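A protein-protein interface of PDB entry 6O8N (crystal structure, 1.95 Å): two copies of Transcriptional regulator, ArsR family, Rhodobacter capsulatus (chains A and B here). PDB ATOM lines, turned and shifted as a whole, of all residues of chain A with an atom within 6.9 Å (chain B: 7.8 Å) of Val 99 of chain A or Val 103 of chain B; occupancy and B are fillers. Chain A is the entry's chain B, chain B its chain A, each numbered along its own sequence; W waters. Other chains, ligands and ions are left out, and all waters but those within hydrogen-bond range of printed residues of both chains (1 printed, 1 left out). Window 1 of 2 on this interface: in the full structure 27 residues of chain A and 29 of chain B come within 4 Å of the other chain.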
ATOM      1  N   ARG A  21       5.522  14.596 -34.936  1.00  0.00           N
ATOM      2  CA  ARG A  21       4.570  14.866 -33.864  1.00  0.00           C
ATOM      3  C   ARG A  21       4.269  16.354 -33.752  1.00  0.00           C
ATOM      4  O   ARG A  21       3.112  16.746 -33.556  1.00  0.00           O
ATOM      5  CB  ARG A  21       5.109  14.330 -32.539  1.00  0.00           C
ATOM      6  CG  ARG A  21       5.083  12.818 -32.433  1.00  0.00           C
ATOM      7  CD  ARG A  21       5.927  12.341 -31.267  1.00  0.00           C
ATOM      8  NE  ARG A  21       5.791  10.904 -31.058  1.00  0.00           N
ATOM      9  CZ  ARG A  21       4.780  10.334 -30.412  1.00  0.00           C
ATOM     10  NH1 ARG A  21       3.803  11.078 -29.905  1.00  0.00           N
ATOM     11  NH2 ARG A  21       4.746   9.018 -30.274  1.00  0.00           N
ATOM     12  N   ALA A  22       5.295  17.199 -33.872  1.00  0.00           N
ATOM     13  CA  ALA A  22       5.071  18.640 -33.842  1.00  0.00           C
ATOM     14  C   ALA A  22       4.269  19.109 -35.048  1.00  0.00           C
ATOM     15  O   ALA A  22       3.483  20.057 -34.937  1.00  0.00           O
ATOM     16  CB  ALA A  22       6.409  19.376 -33.775  1.00  0.00           C
ATOM     17  N   ALA A  25       0.712  18.261 -34.168  1.00  0.00           N
ATOM     18  CA  ALA A  25       0.249  19.298 -33.251  1.00  0.00           C
ATOM     19  C   ALA A  25      -0.019  20.608 -33.981  1.00  0.00           C
ATOM     20  O   ALA A  25      -0.981  21.317 -33.665  1.00  0.00           O
ATOM     21  CB  ALA A  25       1.277  19.504 -32.140  1.00  0.00           C
ATOM     22  N   SER A  26       0.823  20.944 -34.964  1.00  0.00           N
ATOM     23  CA  SER A  26       0.554  22.099 -35.817  1.00  0.00           C
ATOM     24  C   SER A  26      -0.805  21.987 -36.496  1.00  0.00           C
ATOM     25  O   SER A  26      -1.511  22.990 -36.659  1.00  0.00           O
ATOM     26  CB  SER A  26       1.659  22.241 -36.865  1.00  0.00           C
ATOM     27  OG  SER A  26       1.420  23.362 -37.700  1.00  0.00           O
ATOM     28  N   LEU A  28      -3.559  20.417 -35.464  1.00  0.00           N
ATOM     29  CA  LEU A  28      -4.643  20.701 -34.529  1.00  0.00           C
ATOM     30  C   LEU A  28      -4.791  22.199 -34.303  1.00  0.00           C
ATOM     31  O   LEU A  28      -5.907  22.733 -34.307  1.00  0.00           O
ATOM     32  CB  LEU A  28      -4.401  19.982 -33.202  1.00  0.00           C
ATOM     33  CG  LEU A  28      -5.381  20.365 -32.086  1.00  0.00           C
ATOM     34  CD1 LEU A  28      -6.801  19.988 -32.479  1.00  0.00           C
ATOM     35  CD2 LEU A  28      -4.996  19.719 -30.761  1.00  0.00           C
ATOM     36  N   LEU A  29      -3.671  22.896 -34.102  1.00  0.00           N
ATOM     37  CA  LEU A  29      -3.731  24.326 -33.819  1.00  0.00           C
ATOM     38  C   LEU A  29      -4.282  25.101 -35.008  1.00  0.00           C
ATOM     39  O   LEU A  29      -5.022  26.076 -34.833  1.00  0.00           O
ATOM     40  CB  LEU A  29      -2.343  24.841 -33.432  1.00  0.00           C
ATOM     41  CG  LEU A  29      -1.687  24.189 -32.212  1.00  0.00           C
ATOM     42  CD1 LEU A  29      -0.449  24.968 -31.785  1.00  0.00           C
ATOM     43  CD2 LEU A  29      -2.680  24.073 -31.064  1.00  0.00           C
ATOM     44  N   LEU A  32      -7.951  24.752 -34.700  1.00  0.00           N
ATOM     45  CA  LEU A  32      -8.516  25.550 -33.618  1.00  0.00           C
ATOM     46  C   LEU A  32      -8.426  27.047 -33.878  1.00  0.00           C
ATOM     47  O   LEU A  32      -9.220  27.806 -33.313  1.00  0.00           O
ATOM     48  CB  LEU A  32      -7.816  25.221 -32.299  1.00  0.00           C
ATOM     49  CG  LEU A  32      -7.975  23.793 -31.776  1.00  0.00           C
ATOM     50  CD1 LEU A  32      -7.163  23.592 -30.509  1.00  0.00           C
ATOM     51  CD2 LEU A  32      -9.441  23.461 -31.532  1.00  0.00           C
ATOM     52  N   PRO A  94     -10.585  13.973 -26.857  1.00  0.00           N
ATOM     53  CA  PRO A  94      -9.966  14.276 -25.557  1.00  0.00           C
ATOM     54  C   PRO A  94      -8.582  14.888 -25.678  1.00  0.00           C
ATOM     55  O   PRO A  94      -8.152  15.603 -24.765  1.00  0.00           O
ATOM     56  CB  PRO A  94      -9.918  12.907 -24.865  1.00  0.00           C
ATOM     57  CG  PRO A  94      -9.846  11.930 -25.994  1.00  0.00           C
ATOM     58  CD  PRO A  94     -10.660  12.523 -27.113  1.00  0.00           C
ATOM     59  N   ARG A  95      -7.869  14.625 -26.776  1.00  0.00           N
ATOM     60  CA  ARG A  95      -6.615  15.326 -27.031  1.00  0.00           C
ATOM     61  C   ARG A  95      -6.859  16.808 -27.290  1.00  0.00           C
ATOM     62  O   ARG A  95      -6.244  17.671 -26.652  1.00  0.00           O
ATOM     63  CB  ARG A  95      -5.888  14.682 -28.212  1.00  0.00           C
ATOM     64  CG  ARG A  95      -4.493  15.234 -28.460  1.00  0.00           C
ATOM     65  CD  ARG A  95      -3.777  14.450 -29.546  1.00  0.00           C
ATOM     66  NE  ARG A  95      -4.547  14.413 -30.786  1.00  0.00           N
ATOM     67  CZ  ARG A  95      -4.182  13.743 -31.873  1.00  0.00           C
ATOM     68  NH1 ARG A  95      -3.053  13.047 -31.879  1.00  0.00           N
ATOM     69  NH2 ARG A  95      -4.946  13.767 -32.957  1.00  0.00           N
ATOM     70  N   ALA A  96      -7.758  17.121 -28.228  1.00  0.00           N
ATOM     71  CA  ALA A  96      -8.065  18.515 -28.524  1.00  0.00           C
ATOM     72  C   ALA A  96      -8.772  19.198 -27.363  1.00  0.00           C
ATOM     73  O   ALA A  96      -8.603  20.406 -27.163  1.00  0.00           O
ATOM     74  CB  ALA A  96      -8.916  18.607 -29.791  1.00  0.00           C
ATOM     75  N   ALA A  97      -9.561  18.448 -26.588  1.00  0.00           N
ATOM     76  CA  ALA A  97     -10.199  19.023 -25.408  1.00  0.00           C
ATOM     77  C   ALA A  97      -9.165  19.534 -24.412  1.00  0.00           C
ATOM     78  O   ALA A  97      -9.347  20.601 -23.813  1.00  0.00           O
ATOM     79  CB  ALA A  97     -11.113  17.992 -24.749  1.00  0.00           C
ATOM     80  N   ARG A  98      -8.073  18.789 -24.226  1.00  0.00           N
ATOM     81  CA  ARG A  98      -7.052  19.198 -23.265  1.00  0.00           C
ATOM     82  C   ARG A  98      -6.388  20.502 -23.688  1.00  0.00           C
ATOM     83  O   ARG A  98      -6.207  21.410 -22.869  1.00  0.00           O
ATOM     84  CB  ARG A  98      -6.004  18.096 -23.103  1.00  0.00           C
ATOM     85  CG  ARG A  98      -5.249  18.166 -21.789  1.00  0.00           C
ATOM     86  CD  ARG A  98      -5.861  17.217 -20.784  1.00  0.00           C
ATOM     87  NE  ARG A  98      -6.176  15.942 -21.420  1.00  0.00           N
ATOM     88  CZ  ARG A  98      -6.933  14.996 -20.877  1.00  0.00           C
ATOM     89  NH1 ARG A  98      -7.472  15.174 -19.677  1.00  0.00           N
ATOM     90  NH2 ARG A  98      -7.163  13.875 -21.545  1.00  0.00           N
ATOM     91  N   VAL A  99      -6.019  20.609 -24.967  1.00  0.00           N
ATOM     92  CA  VAL A  99      -5.458  21.857 -25.480  1.00  0.00           C
ATOM     93  C   VAL A  99      -6.442  23.001 -25.276  1.00  0.00           C
ATOM     94  O   VAL A  99      -6.075  24.085 -24.809  1.00  0.00           O
ATOM     95  CB  VAL A  99      -5.077  21.704 -26.963  1.00  0.00           C
ATOM     96  CG1 VAL A  99      -4.560  23.024 -27.512  1.00  0.00           C
ATOM     97  CG2 VAL A  99      -4.042  20.599 -27.139  1.00  0.00           C
ATOM     98  N   VAL A 100      -7.713  22.767 -25.611  1.00  0.00           N
ATOM     99  CA  VAL A 100      -8.716  23.826 -25.544  1.00  0.00           C
ATOM    100  C   VAL A 100      -8.917  24.282 -24.103  1.00  0.00           C
ATOM    101  O   VAL A 100      -9.120  25.474 -23.836  1.00  0.00           O
ATOM    102  CB  VAL A 100     -10.034  23.345 -26.183  1.00  0.00           C
ATOM    103  CG1 VAL A 100     -11.204  24.220 -25.753  1.00  0.00           C
ATOM    104  CG2 VAL A 100      -9.910  23.334 -27.697  1.00  0.00           C
ATOM    105  N   GLN A 101      -8.844  23.350 -23.149  1.00  0.00           N
ATOM    106  CA  GLN A 101      -9.021  23.722 -21.748  1.00  0.00           C
ATOM    107  C   GLN A 101      -7.895  24.631 -21.267  1.00  0.00           C
ATOM    108  O   GLN A 101      -8.139  25.586 -20.520  1.00  0.00           O
ATOM    109  CB  GLN A 101      -9.111  22.472 -20.873  1.00  0.00           C
ATOM    110  CG  GLN A 101     -10.411  21.693 -21.021  1.00  0.00           C
ATOM    111  CD  GLN A 101     -11.616  22.422 -20.445  1.00  0.00           C
ATOM    112  OE1 GLN A 101     -11.481  23.438 -19.765  1.00  0.00           O
ATOM    113  NE2 GLN A 101     -12.805  21.897 -20.717  1.00  0.00           N
ATOM    114  N   THR A 102      -6.655  24.354 -21.682  1.00  0.00           N
ATOM    115  CA  THR A 102      -5.554  25.252 -21.348  1.00  0.00           C
ATOM    116  C   THR A 102      -5.733  26.612 -22.010  1.00  0.00           C
ATOM    117  O   THR A 102      -5.531  27.652 -21.372  1.00  0.00           O
ATOM    118  CB  THR A 102      -4.219  24.628 -21.758  1.00  0.00           C
ATOM    119  OG1 THR A 102      -4.065  23.359 -21.113  1.00  0.00           O
ATOM    120  CG2 THR A 102      -3.060  25.533 -21.362  1.00  0.00           C
ATOM    121  N   VAL A 103      -6.122  26.625 -23.287  1.00  0.00           N
ATOM    122  CA  VAL A 103      -6.476  27.880 -23.948  1.00  0.00           C
ATOM    123  C   VAL A 103      -7.594  28.586 -23.191  1.00  0.00           C
ATOM    124  O   VAL A 103      -7.553  29.805 -22.983  1.00  0.00           O
ATOM    125  CB  VAL A 103      -6.859  27.617 -25.417  1.00  0.00           C
ATOM    126  CG1 VAL A 103      -7.276  28.912 -26.101  1.00  0.00           C
ATOM    127  CG2 VAL A 103      -5.702  26.964 -26.159  1.00  0.00           C
ATOM    128  N   TYR A 104      -8.602  27.826 -22.751  1.00  0.00           N
ATOM    129  CA  TYR A 104      -9.691  28.406 -21.973  1.00  0.00           C
ATOM    130  C   TYR A 104      -9.186  28.982 -20.656  1.00  0.00           C
ATOM    131  O   TYR A 104      -9.588  30.081 -20.256  1.00  0.00           O
ATOM    132  CB  TYR A 104     -10.769  27.353 -21.721  1.00  0.00           C
ATOM    133  CG  TYR A 104     -11.864  27.801 -20.780  1.00  0.00           C
ATOM    134  CD1 TYR A 104     -12.915  28.586 -21.231  1.00  0.00           C
ATOM    135  CD2 TYR A 104     -11.847  27.437 -19.438  1.00  0.00           C
ATOM    136  CE1 TYR A 104     -13.917  29.000 -20.376  1.00  0.00           C
ATOM    137  CE2 TYR A 104     -12.845  27.845 -18.575  1.00  0.00           C
ATOM    138  CZ  TYR A 104     -13.878  28.627 -19.050  1.00  0.00           C
ATOM    139  OH  TYR A 104     -14.875  29.036 -18.194  1.00  0.00           O
ATOM    140  N   GLU A 105      -8.302  28.254 -19.969  1.00  0.00           N
ATOM    141  CA  GLU A 105      -7.782  28.733 -18.692  1.00  0.00           C
ATOM    142  C   GLU A 105      -6.954  29.999 -18.871  1.00  0.00           C
ATOM    143  O   GLU A 105      -7.001  30.903 -18.028  1.00  0.00           O
ATOM    144  CB  GLU A 105      -6.951  27.640 -18.020  1.00  0.00           C
ATOM    145  CG  GLU A 105      -7.776  26.538 -17.384  1.00  0.00           C
ATOM    146  CD  GLU A 105      -7.042  25.212 -17.329  1.00  0.00           C
ATOM    147  OE1 GLU A 105      -7.622  24.232 -16.817  1.00  0.00           O
ATOM    148  OE2 GLU A 105      -5.884  25.149 -17.794  1.00  0.00           O
ATOM    149  N   LEU B  29      -3.190  31.189 -31.217  1.00  0.00           N
ATOM    150  CA  LEU B  29      -3.167  29.906 -31.909  1.00  0.00           C
ATOM    151  C   LEU B  29      -2.770  30.062 -33.372  1.00  0.00           C
ATOM    152  O   LEU B  29      -2.148  29.159 -33.942  1.00  0.00           O
ATOM    153  CB  LEU B  29      -4.530  29.224 -31.795  1.00  0.00           C
ATOM    154  CG  LEU B  29      -4.953  28.812 -30.382  1.00  0.00           C
ATOM    155  CD1 LEU B  29      -6.296  28.100 -30.406  1.00  0.00           C
ATOM    156  CD2 LEU B  29      -3.887  27.940 -29.735  1.00  0.00           C
ATOM    157  N   LEU B  32       0.931  30.282 -33.257  1.00  0.00           N
ATOM    158  CA  LEU B  32       1.564  29.016 -32.911  1.00  0.00           C
ATOM    159  C   LEU B  32       1.441  27.973 -34.015  1.00  0.00           C
ATOM    160  O   LEU B  32       2.256  27.046 -34.062  1.00  0.00           O
ATOM    161  CB  LEU B  32       0.964  28.461 -31.618  1.00  0.00           C
ATOM    162  CG  LEU B  32       1.270  29.233 -30.331  1.00  0.00           C
ATOM    163  CD1 LEU B  32       0.496  28.646 -29.163  1.00  0.00           C
ATOM    164  CD2 LEU B  32       2.762  29.235 -30.038  1.00  0.00           C
ATOM    165  N   LEU B  38       6.523  26.185 -34.364  1.00  0.00           N
ATOM    166  CA  LEU B  38       6.006  25.311 -33.317  1.00  0.00           C
ATOM    167  C   LEU B  38       7.030  24.243 -32.947  1.00  0.00           C
ATOM    168  O   LEU B  38       7.122  23.836 -31.792  1.00  0.00           O
ATOM    169  CB  LEU B  38       4.694  24.652 -33.748  1.00  0.00           C
ATOM    170  CG  LEU B  38       3.961  23.890 -32.640  1.00  0.00           C
ATOM    171  CD1 LEU B  38       3.551  24.831 -31.520  1.00  0.00           C
ATOM    172  CD2 LEU B  38       2.754  23.155 -33.190  1.00  0.00           C
ATOM    173  N   CSS B  42       8.149  23.551 -29.301  1.00  0.00           N
ATOM    174  CA  CSS B  42       8.006  22.236 -28.705  1.00  0.00           C
ATOM    175  CB  CSS B  42       7.553  21.220 -29.750  1.00  0.00           C
ATOM    176  SG  CSS B  42       5.887  21.551 -30.224  1.00  0.00           S
ATOM    177  SD  CSS B  42       4.887  20.394 -28.906  1.00  0.00           S
ATOM    178  C   CSS B  42       9.304  21.805 -28.089  1.00  0.00           C
ATOM    179  O   CSS B  42       9.294  21.119 -27.044  1.00  0.00           O
ATOM    180  N   ALA B  45       9.907  23.568 -24.826  1.00  0.00           N
ATOM    181  CA  ALA B  45       8.977  23.203 -23.764  1.00  0.00           C
ATOM    182  C   ALA B  45       9.601  22.229 -22.775  1.00  0.00           C
ATOM    183  O   ALA B  45       9.293  22.281 -21.578  1.00  0.00           O
ATOM    184  CB  ALA B  45       7.702  22.606 -24.361  1.00  0.00           C
ATOM    185  N   ALA B  96       1.235  31.604 -23.665  1.00  0.00           N
ATOM    186  CA  ALA B  96       1.671  30.773 -24.783  1.00  0.00           C
ATOM    187  C   ALA B  96       2.452  29.558 -24.301  1.00  0.00           C
ATOM    188  O   ALA B  96       2.289  28.455 -24.836  1.00  0.00           O
ATOM    189  CB  ALA B  96       2.513  31.601 -25.753  1.00  0.00           C
ATOM    190  N   ALA B  97       3.305  29.738 -23.290  1.00  0.00           N
ATOM    191  CA  ALA B  97       4.080  28.615 -22.772  1.00  0.00           C
ATOM    192  C   ALA B  97       3.176  27.562 -22.143  1.00  0.00           C
ATOM    193  O   ALA B  97       3.438  26.360 -22.257  1.00  0.00           O
ATOM    194  CB  ALA B  97       5.115  29.110 -21.761  1.00  0.00           C
ATOM    195  N   ARG B  98       2.100  27.994 -21.483  1.00  0.00           N
ATOM    196  CA  ARG B  98       1.146  27.041 -20.922  1.00  0.00           C
ATOM    197  C   ARG B  98       0.449  26.248 -22.020  1.00  0.00           C
ATOM    198  O   ARG B  98       0.317  25.021 -21.925  1.00  0.00           O
ATOM    199  CB  ARG B  98       0.121  27.775 -20.057  1.00  0.00           C
ATOM    200  CG  ARG B  98       0.698  28.364 -18.778  1.00  0.00           C
ATOM    201  CD  ARG B  98       0.219  27.615 -17.542  1.00  0.00           C
ATOM    202  NE  ARG B  98       0.664  28.275 -16.319  1.00  0.00           N
ATOM    203  CZ  ARG B  98       1.527  27.746 -15.457  1.00  0.00           C
ATOM    204  NH1 ARG B  98       2.040  26.543 -15.684  1.00  0.00           N
ATOM    205  NH2 ARG B  98       1.882  28.423 -14.373  1.00  0.00           N
ATOM    206  N   VAL B  99      -0.007  26.933 -23.071  1.00  0.00           N
ATOM    207  CA  VAL B  99      -0.610  26.243 -24.208  1.00  0.00           C
ATOM    208  C   VAL B  99       0.377  25.251 -24.807  1.00  0.00           C
ATOM    209  O   VAL B  99       0.034  24.095 -25.081  1.00  0.00           O
ATOM    210  CB  VAL B  99      -1.096  27.261 -25.256  1.00  0.00           C
ATOM    211  CG1 VAL B  99      -1.513  26.548 -26.540  1.00  0.00           C
ATOM    212  CG2 VAL B  99      -2.246  28.084 -24.699  1.00  0.00           C
ATOM    213  N   VAL B 100       1.627  25.682 -24.993  1.00  0.00           N
ATOM    214  CA  VAL B 100       2.612  24.848 -25.675  1.00  0.00           C
ATOM    215  C   VAL B 100       2.933  23.610 -24.844  1.00  0.00           C
ATOM    216  O   VAL B 100       3.094  22.508 -25.384  1.00  0.00           O
ATOM    217  CB  VAL B 100       3.876  25.670 -25.991  1.00  0.00           C
ATOM    218  CG1 VAL B 100       5.032  24.760 -26.382  1.00  0.00           C
ATOM    219  CG2 VAL B 100       3.592  26.674 -27.101  1.00  0.00           C
ATOM    220  N   GLN B 101       3.010  23.763 -23.519  1.00  0.00           N
ATOM    221  CA  GLN B 101       3.311  22.622 -22.660  1.00  0.00           C
ATOM    222  C   GLN B 101       2.201  21.579 -22.711  1.00  0.00           C
ATOM    223  O   GLN B 101       2.476  20.375 -22.750  1.00  0.00           O
ATOM    224  CB  GLN B 101       3.541  23.084 -21.220  1.00  0.00           C
ATOM    225  CG  GLN B 101       4.822  23.877 -21.005  1.00  0.00           C
ATOM    226  CD  GLN B 101       6.073  23.020 -21.061  1.00  0.00           C
ATOM    227  OE1 GLN B 101       6.003  21.794 -21.159  1.00  0.00           O
ATOM    228  NE2 GLN B 101       7.230  23.667 -20.997  1.00  0.00           N
ATOM    229  N   THR B 102       0.940  22.022 -22.706  1.00  0.00           N
ATOM    230  CA  THR B 102      -0.169  21.094 -22.908  1.00  0.00           C
ATOM    231  C   THR B 102      -0.105  20.448 -24.286  1.00  0.00           C
ATOM    232  O   THR B 102      -0.321  19.238 -24.424  1.00  0.00           O
ATOM    233  CB  THR B 102      -1.505  21.815 -22.723  1.00  0.00           C
ATOM    234  OG1 THR B 102      -1.541  22.441 -21.435  1.00  0.00           O
ATOM    235  CG2 THR B 102      -2.663  20.830 -22.840  1.00  0.00           C
ATOM    236  N   VAL B 103       0.189  21.242 -25.318  1.00  0.00           N
ATOM    237  CA  VAL B 103       0.420  20.684 -26.647  1.00  0.00           C
ATOM    238  C   VAL B 103       1.576  19.691 -26.616  1.00  0.00           C
ATOM    239  O   VAL B 103       1.507  18.615 -27.224  1.00  0.00           O
ATOM    240  CB  VAL B 103       0.667  21.815 -27.662  1.00  0.00           C
ATOM    241  CG1 VAL B 103       1.194  21.255 -28.968  1.00  0.00           C
ATOM    242  CG2 VAL B 103      -0.614  22.606 -27.898  1.00  0.00           C
ATOM    243  N   TYR B 104       2.650  20.030 -25.896  1.00  0.00           N
ATOM    244  CA  TYR B 104       3.780  19.116 -25.769  1.00  0.00           C
ATOM    245  C   TYR B 104       3.364  17.807 -25.110  1.00  0.00           C
ATOM    246  O   TYR B 104       3.748  16.724 -25.568  1.00  0.00           O
ATOM    247  CB  TYR B 104       4.907  19.778 -24.974  1.00  0.00           C
ATOM    248  CG  TYR B 104       6.167  18.944 -24.890  1.00  0.00           C
ATOM    249  CD1 TYR B 104       6.391  18.090 -23.817  1.00  0.00           C
ATOM    250  CD2 TYR B 104       7.132  19.010 -25.886  1.00  0.00           C
ATOM    251  CE1 TYR B 104       7.540  17.325 -23.741  1.00  0.00           C
ATOM    252  CE2 TYR B 104       8.282  18.249 -25.818  1.00  0.00           C
ATOM    253  CZ  TYR B 104       8.481  17.410 -24.744  1.00  0.00           C
ATOM    254  OH  TYR B 104       9.629  16.654 -24.676  1.00  0.00           O
ATOM    255  N   GLU B 105       2.582  17.888 -24.034  1.00  0.00           N
ATOM    256  CA  GLU B 105       2.171  16.682 -23.326  1.00  0.00           C
ATOM    257  C   GLU B 105       1.278  15.799 -24.187  1.00  0.00           C
ATOM    258  O   GLU B 105       1.275  14.574 -24.027  1.00  0.00           O
ATOM    259  CB  GLU B 105       1.458  17.058 -22.027  1.00  0.00           C
ATOM    260  CG  GLU B 105       2.366  17.665 -20.967  1.00  0.00           C
ATOM    261  CD  GLU B 105       1.636  18.650 -20.076  1.00  0.00           C
ATOM    262  OE1 GLU B 105       0.390  18.700 -20.141  1.00  0.00           O
ATOM    263  OE2 GLU B 105       2.307  19.372 -19.307  1.00  0.00           O
ATOM    264  N   GLN B 106       0.523  16.397 -25.110  1.00  0.00           N
ATOM    265  CA  GLN B 106      -0.466  15.658 -25.881  1.00  0.00           C
ATOM    266  C   GLN B 106       0.092  15.084 -27.177  1.00  0.00           C
ATOM    267  O   GLN B 106      -0.464  14.108 -27.692  1.00  0.00           O
ATOM    268  CB  GLN B 106      -1.666  16.556 -26.199  1.00  0.00           C
ATOM    269  CG  GLN B 106      -2.518  16.906 -24.988  1.00  0.00           C
ATOM    270  CD  GLN B 106      -3.071  15.680 -24.287  1.00  0.00           C
ATOM    271  OE1 GLN B 106      -3.712  14.833 -24.908  1.00  0.00           O
ATOM    272  NE2 GLN B 106      -2.826  15.582 -22.985  1.00  0.00           N
ATOM    273  N   PHE B 107       1.168  15.654 -27.711  1.00  0.00           N
ATOM    274  CA  PHE B 107       1.651  15.269 -29.032  1.00  0.00           C
ATOM    275  C   PHE B 107       3.096  14.782 -28.986  1.00  0.00           C
ATOM    276  O   PHE B 107       3.488  13.921 -29.770  1.00  0.00           O
ATOM    277  CB  PHE B 107       1.529  16.437 -30.011  1.00  0.00           C
ATOM    278  CG  PHE B 107       0.128  16.680 -30.493  1.00  0.00           C
ATOM    279  CD1 PHE B 107      -0.338  16.070 -31.646  1.00  0.00           C
ATOM    280  CD2 PHE B 107      -0.721  17.523 -29.796  1.00  0.00           C
ATOM    281  CE1 PHE B 107      -1.626  16.295 -32.095  1.00  0.00           C
ATOM    282  CE2 PHE B 107      -2.011  17.752 -30.240  1.00  0.00           C
ATOM    283  CZ  PHE B 107      -2.462  17.137 -31.390  1.00  0.00           C
ATOM    284  N   CSS B 108       3.882  15.335 -28.067  1.00  0.00           N
ATOM    285  CA  CSS B 108       5.330  15.258 -28.150  1.00  0.00           C
ATOM    286  CB  CSS B 108       5.940  16.657 -28.137  1.00  0.00           C
ATOM    287  SG  CSS B 108       6.031  17.313 -29.771  1.00  0.00           S
ATOM    288  SD  CSS B 108       4.479  18.612 -29.745  1.00  0.00           S
ATOM    289  C   CSS B 108       5.878  14.443 -27.010  1.00  0.00           C
ATOM    290  O   CSS B 108       7.079  14.562 -26.685  1.00  0.00           O
ATOM    291  N   SER B 109       5.033  13.622 -26.394  1.00  0.00           N
ATOM    292  CA  SER B 109       5.395  12.933 -25.158  1.00  0.00           C
ATOM    293  C   SER B 109       5.284  11.421 -25.323  1.00  0.00           C
ATOM    294  O   SER B 109       5.077  10.694 -24.350  1.00  0.00           O
ATOM    295  CB  SER B 109       4.508  13.401 -24.002  1.00  0.00           C
ATOM    296  OG  SER B 109       4.911  14.674 -23.528  1.00  0.00           O
HETATM  297  O   HOH W   1      -1.244  12.166 -29.500  1.00  0.00           O
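The side-chain hydroxyl (OG1) of Thr 102 of chain B lies within hydrogen-bond range of the side-chain hydroxyl (OG1) of Thr 102 of chain A (2.7 Å).
The guanidinium group of Arg 21 of chain A is in hydrogen-bond range of the backbone carbonyl oxygen of Phe 107 of chain B (2.9 Å).
Of the printed residues of chain B, Ala 25 of chain A touches Leu 38, Val 103 and Phe 107.
Pro 94 of chain A touches none of the printed residues of chain B.
Printed residues of chain B within 4 Å of Arg 95 of chain A: Gln 106 (3.6 Å) and Phe 107 (3.5 Å).
Of the printed residues of chain B, Val 99 of chain A touches Thr 102 and Val 103.
Printed residues of chain A within 4 Å of Leu 29 of chain B: Leu 32 (3.8 Å).
Ala 97 of chain B touches none of the printed residues of chain A.
Of the printed residues of chain A, Thr 102 of chain B touches Arg 98, Val 99 and Thr 102.
The nearest printed residue of chain B that does not touch Val 99 of chain A is Gln 106 of chain B (4.5 Å).
Among the printed residues, merely in contact across the chains: Ala 22 of chain A with Leu 38 of chain B (3.6 Å), Ala 25 of chain A with Leu 38 of chain B (3.8 Å), Ala 25 of chain A with Val 103 of chain B (3.6 Å), Ala 25 of chain A with Phe 107 of chain B (3.5 Å), Ser 26 of chain A with Leu 38 of chain B (3.4 Å), Leu 28 of chain A with Phe 107 of chain B (3.6 Å), Leu 29 of chain A with Leu 32 of chain B (3.8 Å), Leu 29 of chain A with Leu 38 of chain B (3.9 Å), Leu 32 of chain A with Leu 29 of chain B (3.8 Å), Arg 95 of chain A with Gln 106 of chain B (3.6 Å), Arg 95 of chain A with Phe 107 of chain B (3.5 Å), Arg 98 of chain A with Thr 102 of chain B (3.6 Å), Arg 98 of chain A with Gln 106 of chain B (3.7 Å), Val 99 of chain A with Thr 102 of chain B (3.98 Å), Val 99 of chain A with Val 103 of chain B (3.99 Å), Thr 102 of chain A with Arg 98 of chain B (3.5 Å), Thr 102 of chain A with Val 99 of chain B (3.8 Å) and Val 103 of chain A with Val 99 of chain B (3.9 Å).
Leu 29 of chain A touches Leu 32 of chain B, and with the chains exchanged Leu 32 of chain A touches Leu 29 of chain B.
Arg 98 of chain A touches Thr 102 of chain B, and with the chains exchanged Thr 102 of chain A touches Arg 98 of chain B.
Val 99 of chain A touches Val 103 of chain B, and with the chains exchanged Val 103 of chain A touches Val 99 of chain B.
Thr 102 of chain B touches its own counterpart, Thr 102 of chain A.
Of the 20 pairs that touch across the chains among the printed residues, 9 have their exchanged pair printed and touching as well.
Water W1 bridges O of Gln 106 of chain B and NH1 of Arg 95 of chain A.
OG1 of Thr 102 of chain B is in hydrogen-bond range of O of Arg 98 of chain B, 3.2 Å away.
O of Arg 98 of chain A lies within hydrogen-bond range of OG1 of Thr 102 of chain A (3.4 Å).
Printed residues of chain A that touch a printed residue of chain B: Arg 21, Ala 22, Ala 25, Ser 26, Leu 28, Leu 29, Leu 32, Arg 95, Arg 98, Val 99, Thr 102 and Val 103.
Hydrophobic or aromatic side chains of chain A within 4 Å of the printed part of chain B: Ala 25, Leu 28, Leu 29, Leu 32, Val 99 and Val 103.
Along chain A the printed residues that touch a printed residue of chain B span positions 21 to 103.
Hydrophobic or aromatic side chains of chain B that line the printed part of chain A: Leu 29, Leu 32, Leu 38, Val 99, Val 103 and Phe 107.
Among the printed residues, 20 pairs touch across the chains.
Among the printed residues, no Asp or Glu carboxylate lies within 4 Å of a Lys or Arg side-chain nitrogen of the other chain.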
